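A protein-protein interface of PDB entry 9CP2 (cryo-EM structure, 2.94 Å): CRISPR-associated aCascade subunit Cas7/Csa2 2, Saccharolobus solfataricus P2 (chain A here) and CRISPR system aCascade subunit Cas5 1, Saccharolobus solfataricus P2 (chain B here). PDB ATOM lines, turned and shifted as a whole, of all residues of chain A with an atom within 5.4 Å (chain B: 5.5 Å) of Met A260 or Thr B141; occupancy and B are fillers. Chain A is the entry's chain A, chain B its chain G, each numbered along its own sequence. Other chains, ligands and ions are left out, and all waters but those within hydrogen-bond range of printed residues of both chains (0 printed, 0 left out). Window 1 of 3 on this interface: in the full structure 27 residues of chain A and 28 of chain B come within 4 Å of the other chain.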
ATOM      1  N   SER A   3     -10.144   9.985 -19.781  1.00  0.00           N
ATOM      2  CA  SER A   3      -9.522   9.634 -18.512  1.00  0.00           C
ATOM      3  C   SER A   3     -10.207   8.397 -17.956  1.00  0.00           C
ATOM      4  O   SER A   3     -11.343   8.095 -18.317  1.00  0.00           O
ATOM      5  CB  SER A   3      -9.602  10.788 -17.507  1.00  0.00           C
ATOM      6  OG  SER A   3      -9.002  11.959 -18.032  1.00  0.00           O
ATOM      7  N   LYS A 138      -0.608   9.047 -20.135  1.00  0.00           N
ATOM      8  CA  LYS A 138      -0.029   9.112 -18.804  1.00  0.00           C
ATOM      9  C   LYS A 138      -0.642   8.018 -17.945  1.00  0.00           C
ATOM     10  O   LYS A 138      -1.869   7.860 -17.914  1.00  0.00           O
ATOM     11  CB  LYS A 138      -0.260  10.488 -18.180  1.00  0.00           C
ATOM     12  CG  LYS A 138       0.000  11.631 -19.143  1.00  0.00           C
ATOM     13  CD  LYS A 138      -0.126  12.976 -18.466  1.00  0.00           C
ATOM     14  CE  LYS A 138      -0.278  14.078 -19.493  1.00  0.00           C
ATOM     15  NZ  LYS A 138      -1.105  15.199 -18.978  1.00  0.00           N
ATOM     16  N   GLU A 189      -4.673   8.689 -18.197  1.00  0.00           N
ATOM     17  CA  GLU A 189      -5.141   9.824 -18.980  1.00  0.00           C
ATOM     18  C   GLU A 189      -4.573   9.738 -20.390  1.00  0.00           C
ATOM     19  O   GLU A 189      -3.426   9.326 -20.574  1.00  0.00           O
ATOM     20  CB  GLU A 189      -4.729  11.147 -18.322  1.00  0.00           C
ATOM     21  CG  GLU A 189      -4.677  12.332 -19.266  1.00  0.00           C
ATOM     22  CD  GLU A 189      -4.197  13.595 -18.589  1.00  0.00           C
ATOM     23  OE1 GLU A 189      -4.333  13.695 -17.352  1.00  0.00           O
ATOM     24  OE2 GLU A 189      -3.682  14.487 -19.294  1.00  0.00           O
ATOM     25  N   PRO A 258      -9.939  19.590 -19.316  1.00  0.00           N
ATOM     26  CA  PRO A 258      -9.190  18.750 -18.373  1.00  0.00           C
ATOM     27  C   PRO A 258     -10.061  18.295 -17.212  1.00  0.00           C
ATOM     28  O   PRO A 258     -10.809  19.080 -16.626  1.00  0.00           O
ATOM     29  CB  PRO A 258      -8.060  19.671 -17.903  1.00  0.00           C
ATOM     30  CG  PRO A 258      -7.898  20.652 -19.002  1.00  0.00           C
ATOM     31  CD  PRO A 258      -9.269  20.880 -19.553  1.00  0.00           C
ATOM     32  N   PHE A 259      -9.940  17.014 -16.872  1.00  0.00           N
ATOM     33  CA  PHE A 259     -10.740  16.387 -15.830  1.00  0.00           C
ATOM     34  C   PHE A 259     -10.208  14.984 -15.585  1.00  0.00           C
ATOM     35  O   PHE A 259      -9.729  14.325 -16.511  1.00  0.00           O
ATOM     36  CB  PHE A 259     -12.221  16.328 -16.219  1.00  0.00           C
ATOM     37  CG  PHE A 259     -13.095  15.707 -15.173  1.00  0.00           C
ATOM     38  CD1 PHE A 259     -13.341  16.361 -13.981  1.00  0.00           C
ATOM     39  CD2 PHE A 259     -13.668  14.468 -15.383  1.00  0.00           C
ATOM     40  CE1 PHE A 259     -14.145  15.788 -13.019  1.00  0.00           C
ATOM     41  CE2 PHE A 259     -14.471  13.891 -14.426  1.00  0.00           C
ATOM     42  CZ  PHE A 259     -14.709  14.551 -13.242  1.00  0.00           C
ATOM     43  N   MET A 260     -10.304  14.533 -14.332  1.00  0.00           N
ATOM     44  CA  MET A 260      -9.898  13.186 -13.951  1.00  0.00           C
ATOM     45  C   MET A 260     -10.789  12.679 -12.826  1.00  0.00           C
ATOM     46  O   MET A 260     -11.056  13.415 -11.866  1.00  0.00           O
ATOM     47  CB  MET A 260      -8.432  13.129 -13.504  1.00  0.00           C
ATOM     48  CG  MET A 260      -7.436  13.174 -14.646  1.00  0.00           C
ATOM     49  SD  MET A 260      -5.786  12.716 -14.108  1.00  0.00           S
ATOM     50  CE  MET A 260      -5.724  13.581 -12.546  1.00  0.00           C
ATOM     51  N   PRO A 261     -11.257  11.437 -12.915  1.00  0.00           N
ATOM     52  CA  PRO A 261     -12.166  10.911 -11.891  1.00  0.00           C
ATOM     53  C   PRO A 261     -11.455  10.688 -10.564  1.00  0.00           C
ATOM     54  O   PRO A 261     -10.243  10.858 -10.424  1.00  0.00           O
ATOM     55  CB  PRO A 261     -12.661   9.589 -12.484  1.00  0.00           C
ATOM     56  CG  PRO A 261     -11.712   9.254 -13.569  1.00  0.00           C
ATOM     57  CD  PRO A 261     -11.100  10.523 -14.056  1.00  0.00           C
ATOM     58  N   GLU A 262     -12.252  10.305  -9.570  1.00  0.00           N
ATOM     59  CA  GLU A 262     -11.726  10.030  -8.245  1.00  0.00           C
ATOM     60  C   GLU A 262     -10.901   8.745  -8.247  1.00  0.00           C
ATOM     61  O   GLU A 262     -11.193   7.812  -8.999  1.00  0.00           O
ATOM     62  CB  GLU A 262     -12.864   9.906  -7.234  1.00  0.00           C
ATOM     63  CG  GLU A 262     -13.645  11.188  -7.015  1.00  0.00           C
ATOM     64  CD  GLU A 262     -12.990  12.093  -5.992  1.00  0.00           C
ATOM     65  OE1 GLU A 262     -11.962  11.687  -5.413  1.00  0.00           O
ATOM     66  OE2 GLU A 262     -13.496  13.213  -5.770  1.00  0.00           O
ATOM     67  N   THR A 273     -17.232  11.134  -8.520  1.00  0.00           N
ATOM     68  CA  THR A 273     -16.725  11.632  -9.792  1.00  0.00           C
ATOM     69  C   THR A 273     -17.852  12.145 -10.677  1.00  0.00           C
ATOM     70  O   THR A 273     -17.644  13.093 -11.435  1.00  0.00           O
ATOM     71  CB  THR A 273     -15.910  10.560 -10.518  1.00  0.00           C
ATOM     72  OG1 THR A 273     -15.375  11.112 -11.725  1.00  0.00           O
ATOM     73  CG2 THR A 273     -16.764   9.360 -10.863  1.00  0.00           C
ATOM     74  N   ARG A 276     -18.526  15.646  -9.293  1.00  0.00           N
ATOM     75  CA  ARG A 276     -17.447  16.553  -9.662  1.00  0.00           C
ATOM     76  C   ARG A 276     -17.469  16.862 -11.152  1.00  0.00           C
ATOM     77  O   ARG A 276     -17.184  17.992 -11.560  1.00  0.00           O
ATOM     78  CB  ARG A 276     -16.100  15.965  -9.252  1.00  0.00           C
ATOM     79  CG  ARG A 276     -15.911  15.848  -7.751  1.00  0.00           C
ATOM     80  CD  ARG A 276     -14.443  15.906  -7.367  1.00  0.00           C
ATOM     81  NE  ARG A 276     -13.635  14.959  -8.122  1.00  0.00           N
ATOM     82  CZ  ARG A 276     -12.779  15.299  -9.077  1.00  0.00           C
ATOM     83  NH1 ARG A 276     -12.596  16.563  -9.421  1.00  0.00           N
ATOM     84  NH2 ARG A 276     -12.092  14.349  -9.703  1.00  0.00           N
ATOM     85  N   HIS B  11      -3.649  10.814  -6.149  1.00  0.00           N
ATOM     86  CA  HIS B  11      -3.959   9.425  -6.470  1.00  0.00           C
ATOM     87  C   HIS B  11      -3.030   8.466  -5.738  1.00  0.00           C
ATOM     88  O   HIS B  11      -3.479   7.638  -4.938  1.00  0.00           O
ATOM     89  CB  HIS B  11      -3.876   9.206  -7.980  1.00  0.00           C
ATOM     90  CG  HIS B  11      -5.104   9.635  -8.718  1.00  0.00           C
ATOM     91  ND1 HIS B  11      -6.134   8.768  -9.013  1.00  0.00           N
ATOM     92  CD2 HIS B  11      -5.466  10.837  -9.223  1.00  0.00           C
ATOM     93  CE1 HIS B  11      -7.080   9.419  -9.665  1.00  0.00           C
ATOM     94  NE2 HIS B  11      -6.700  10.676  -9.806  1.00  0.00           N
ATOM     95  N   ALA B  39       1.494  23.801 -12.377  1.00  0.00           N
ATOM     96  CA  ALA B  39       0.241  23.054 -12.405  1.00  0.00           C
ATOM     97  C   ALA B  39      -0.938  23.983 -12.650  1.00  0.00           C
ATOM     98  O   ALA B  39      -1.913  23.602 -13.306  1.00  0.00           O
ATOM     99  CB  ALA B  39       0.058  22.282 -11.100  1.00  0.00           C
ATOM    100  N   TYR B  42      -0.928  25.019 -16.414  1.00  0.00           N
ATOM    101  CA  TYR B  42      -1.340  23.961 -17.335  1.00  0.00           C
ATOM    102  C   TYR B  42      -2.719  24.224 -17.927  1.00  0.00           C
ATOM    103  O   TYR B  42      -2.973  23.871 -19.083  1.00  0.00           O
ATOM    104  CB  TYR B  42      -1.326  22.606 -16.625  1.00  0.00           C
ATOM    105  CG  TYR B  42      -2.047  21.491 -17.364  1.00  0.00           C
ATOM    106  CD1 TYR B  42      -3.409  21.272 -17.186  1.00  0.00           C
ATOM    107  CD2 TYR B  42      -1.365  20.657 -18.233  1.00  0.00           C
ATOM    108  CE1 TYR B  42      -4.063  20.260 -17.857  1.00  0.00           C
ATOM    109  CE2 TYR B  42      -2.013  19.640 -18.906  1.00  0.00           C
ATOM    110  CZ  TYR B  42      -3.361  19.446 -18.714  1.00  0.00           C
ATOM    111  OH  TYR B  42      -4.011  18.436 -19.381  1.00  0.00           O
ATOM    112  N   SER B 139      -8.748  23.356 -13.174  1.00  0.00           N
ATOM    113  CA  SER B 139      -8.161  22.649 -14.310  1.00  0.00           C
ATOM    114  C   SER B 139      -6.760  22.148 -13.971  1.00  0.00           C
ATOM    115  O   SER B 139      -5.805  22.337 -14.728  1.00  0.00           O
ATOM    116  CB  SER B 139      -8.129  23.545 -15.544  1.00  0.00           C
ATOM    117  OG  SER B 139      -9.420  24.040 -15.847  1.00  0.00           O
ATOM    118  N   ILE B 140      -6.621  21.504 -12.816  1.00  0.00           N
ATOM    119  CA  ILE B 140      -5.341  20.985 -12.346  1.00  0.00           C
ATOM    120  C   ILE B 140      -5.401  19.464 -12.353  1.00  0.00           C
ATOM    121  O   ILE B 140      -6.357  18.870 -11.837  1.00  0.00           O
ATOM    122  CB  ILE B 140      -5.006  21.525 -10.946  1.00  0.00           C
ATOM    123  CG1 ILE B 140      -4.419  22.934 -11.055  1.00  0.00           C
ATOM    124  CG2 ILE B 140      -4.045  20.598 -10.225  1.00  0.00           C
ATOM    125  CD1 ILE B 140      -4.330  23.668  -9.739  1.00  0.00           C
ATOM    126  N   THR B 141      -4.386  18.828 -12.946  1.00  0.00           N
ATOM    127  CA  THR B 141      -4.379  17.383 -13.122  1.00  0.00           C
ATOM    128  C   THR B 141      -3.137  16.675 -12.598  1.00  0.00           C
ATOM    129  O   THR B 141      -3.239  15.502 -12.228  1.00  0.00           O
ATOM    130  CB  THR B 141      -4.540  17.018 -14.607  1.00  0.00           C
ATOM    131  OG1 THR B 141      -3.441  17.555 -15.354  1.00  0.00           O
ATOM    132  CG2 THR B 141      -5.850  17.553 -15.159  1.00  0.00           C
ATOM    133  N   ARG B 142      -1.980  17.327 -12.554  1.00  0.00           N
ATOM    134  CA  ARG B 142      -0.807  16.634 -12.042  1.00  0.00           C
ATOM    135  C   ARG B 142       0.144  17.631 -11.402  1.00  0.00           C
ATOM    136  O   ARG B 142       0.282  18.768 -11.861  1.00  0.00           O
ATOM    137  CB  ARG B 142      -0.088  15.839 -13.139  1.00  0.00           C
ATOM    138  CG  ARG B 142       0.681  16.674 -14.142  1.00  0.00           C
ATOM    139  CD  ARG B 142       1.366  15.800 -15.176  1.00  0.00           C
ATOM    140  NE  ARG B 142       2.245  16.559 -16.058  1.00  0.00           N
ATOM    141  CZ  ARG B 142       3.526  16.801 -15.813  1.00  0.00           C
ATOM    142  NH1 ARG B 142       4.105  16.395 -14.698  1.00  0.00           N
ATOM    143  NH2 ARG B 142       4.241  17.473 -16.709  1.00  0.00           N
ATOM    144  N   ILE B 143       0.792  17.184 -10.329  1.00  0.00           N
ATOM    145  CA  ILE B 143       1.775  17.969  -9.595  1.00  0.00           C
ATOM    146  C   ILE B 143       3.059  17.157  -9.524  1.00  0.00           C
ATOM    147  O   ILE B 143       3.069  16.059  -8.956  1.00  0.00           O
ATOM    148  CB  ILE B 143       1.284  18.330  -8.184  1.00  0.00           C
ATOM    149  CG1 ILE B 143       0.228  19.434  -8.251  1.00  0.00           C
ATOM    150  CG2 ILE B 143       2.445  18.750  -7.303  1.00  0.00           C
ATOM    151  CD1 ILE B 143      -0.567  19.587  -6.983  1.00  0.00           C
ATOM    152  N   CYS B 148       2.185  11.485 -11.344  1.00  0.00           N
ATOM    153  CA  CYS B 148       1.562  12.057 -10.151  1.00  0.00           C
ATOM    154  C   CYS B 148       0.240  12.731 -10.517  1.00  0.00           C
ATOM    155  O   CYS B 148       0.090  13.952 -10.485  1.00  0.00           O
ATOM    156  CB  CYS B 148       2.517  13.030  -9.474  1.00  0.00           C
ATOM    157  SG  CYS B 148       4.202  12.423  -9.330  1.00  0.00           S
ATOM    158  N   LEU B 149      -0.733  11.898 -10.865  1.00  0.00           N
ATOM    159  CA  LEU B 149      -2.077  12.394 -11.116  1.00  0.00           C
ATOM    160  C   LEU B 149      -2.684  12.941  -9.829  1.00  0.00           C
ATOM    161  O   LEU B 149      -2.329  12.524  -8.723  1.00  0.00           O
ATOM    162  CB  LEU B 149      -2.961  11.287 -11.687  1.00  0.00           C
ATOM    163  CG  LEU B 149      -2.402  10.523 -12.887  1.00  0.00           C
ATOM    164  CD1 LEU B 149      -3.324   9.382 -13.270  1.00  0.00           C
ATOM    165  CD2 LEU B 149      -2.189  11.459 -14.062  1.00  0.00           C
ATOM    166  N   ALA B 150      -3.609  13.886  -9.979  1.00  0.00           N
ATOM    167  CA  ALA B 150      -4.212  14.548  -8.827  1.00  0.00           C
ATOM    168  C   ALA B 150      -5.562  15.121  -9.223  1.00  0.00           C
ATOM    169  O   ALA B 150      -5.643  15.931 -10.149  1.00  0.00           O
ATOM    170  CB  ALA B 150      -3.296  15.652  -8.295  1.00  0.00           C
ATOM    171  N   SER B 151      -6.611  14.702  -8.523  1.00  0.00           N
ATOM    172  CA  SER B 151      -7.940  15.247  -8.742  1.00  0.00           C
ATOM    173  C   SER B 151      -8.119  16.549  -7.964  1.00  0.00           C
ATOM    174  O   SER B 151      -7.389  16.842  -7.016  1.00  0.00           O
ATOM    175  CB  SER B 151      -9.011  14.240  -8.327  1.00  0.00           C
ATOM    176  OG  SER B 151      -8.774  12.970  -8.907  1.00  0.00           O
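O of Pro A261 is in hydrogen-bond range of OG of Ser B151, at 3.0 Å.
NH2 of Arg A276 is in hydrogen-bond range of O of Met A260 (2.6 Å).
A ring nitrogen (NE2) of His B11 is in hydrogen-bond range of the side-chain hydroxyl (OG) of Ser B151.
The side-chain amino group of Lys A138 is in salt-bridge range of the side-chain carboxylate of Glu A189 (2.7 Å).
The backbone NH (N) of Ala B150 lies within hydrogen-bond range of the backbone carbonyl oxygen (O) of Thr B141.
N of His B11 lies within hydrogen-bond range of O of Leu B149.
The side-chain carboxylate (OE2) of Glu A262 lies within salt-bridge range of the guanidinium group (NE) of Arg A276 (2.9 Å).
Among the printed residues, merely in contact across the chains: Glu A189 with Tyr B42 (3.96 Å), Met A260 with Thr B141 (3.2 Å), Met A260 with Leu B149 (3.7 Å), Met A260 with Ala B150 (3.3 Å), Met A260 with Ser B151 (3.8 Å), Pro A261 with His B11 (3.6 Å) and Arg A276 with Ser B151 (3.4 Å).
Of chain B, only Thr B141 (3.2 Å), Leu B149 (3.7 Å), Ala B150 (3.3 Å) and Ser B151 (3.8 Å) come within 4 Å of Met A260.
Thr B141 touches just one residue of chain A: Met A260 (3.2 Å).
Of the printed residues of chain A, Ala B150 touches Met A260.
Of the printed residues of chain A, Ser B151 touches Met A260 (3.8 Å), Pro A261 (3.0 Å) and Arg A276 (3.4 Å).
The nearest residue of chain A that does not touch Thr B141 is Pro A258 (4.1 Å).
Printed residues of chain B that touch a printed residue of chain A: His B11, Tyr B42, Thr B141, Leu B149, Ala B150 and Ser B151.
Hydrophobic or aromatic side chains of chain B within 4 Å of the printed part of chain A: His B11, Tyr B42 and Leu B149.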
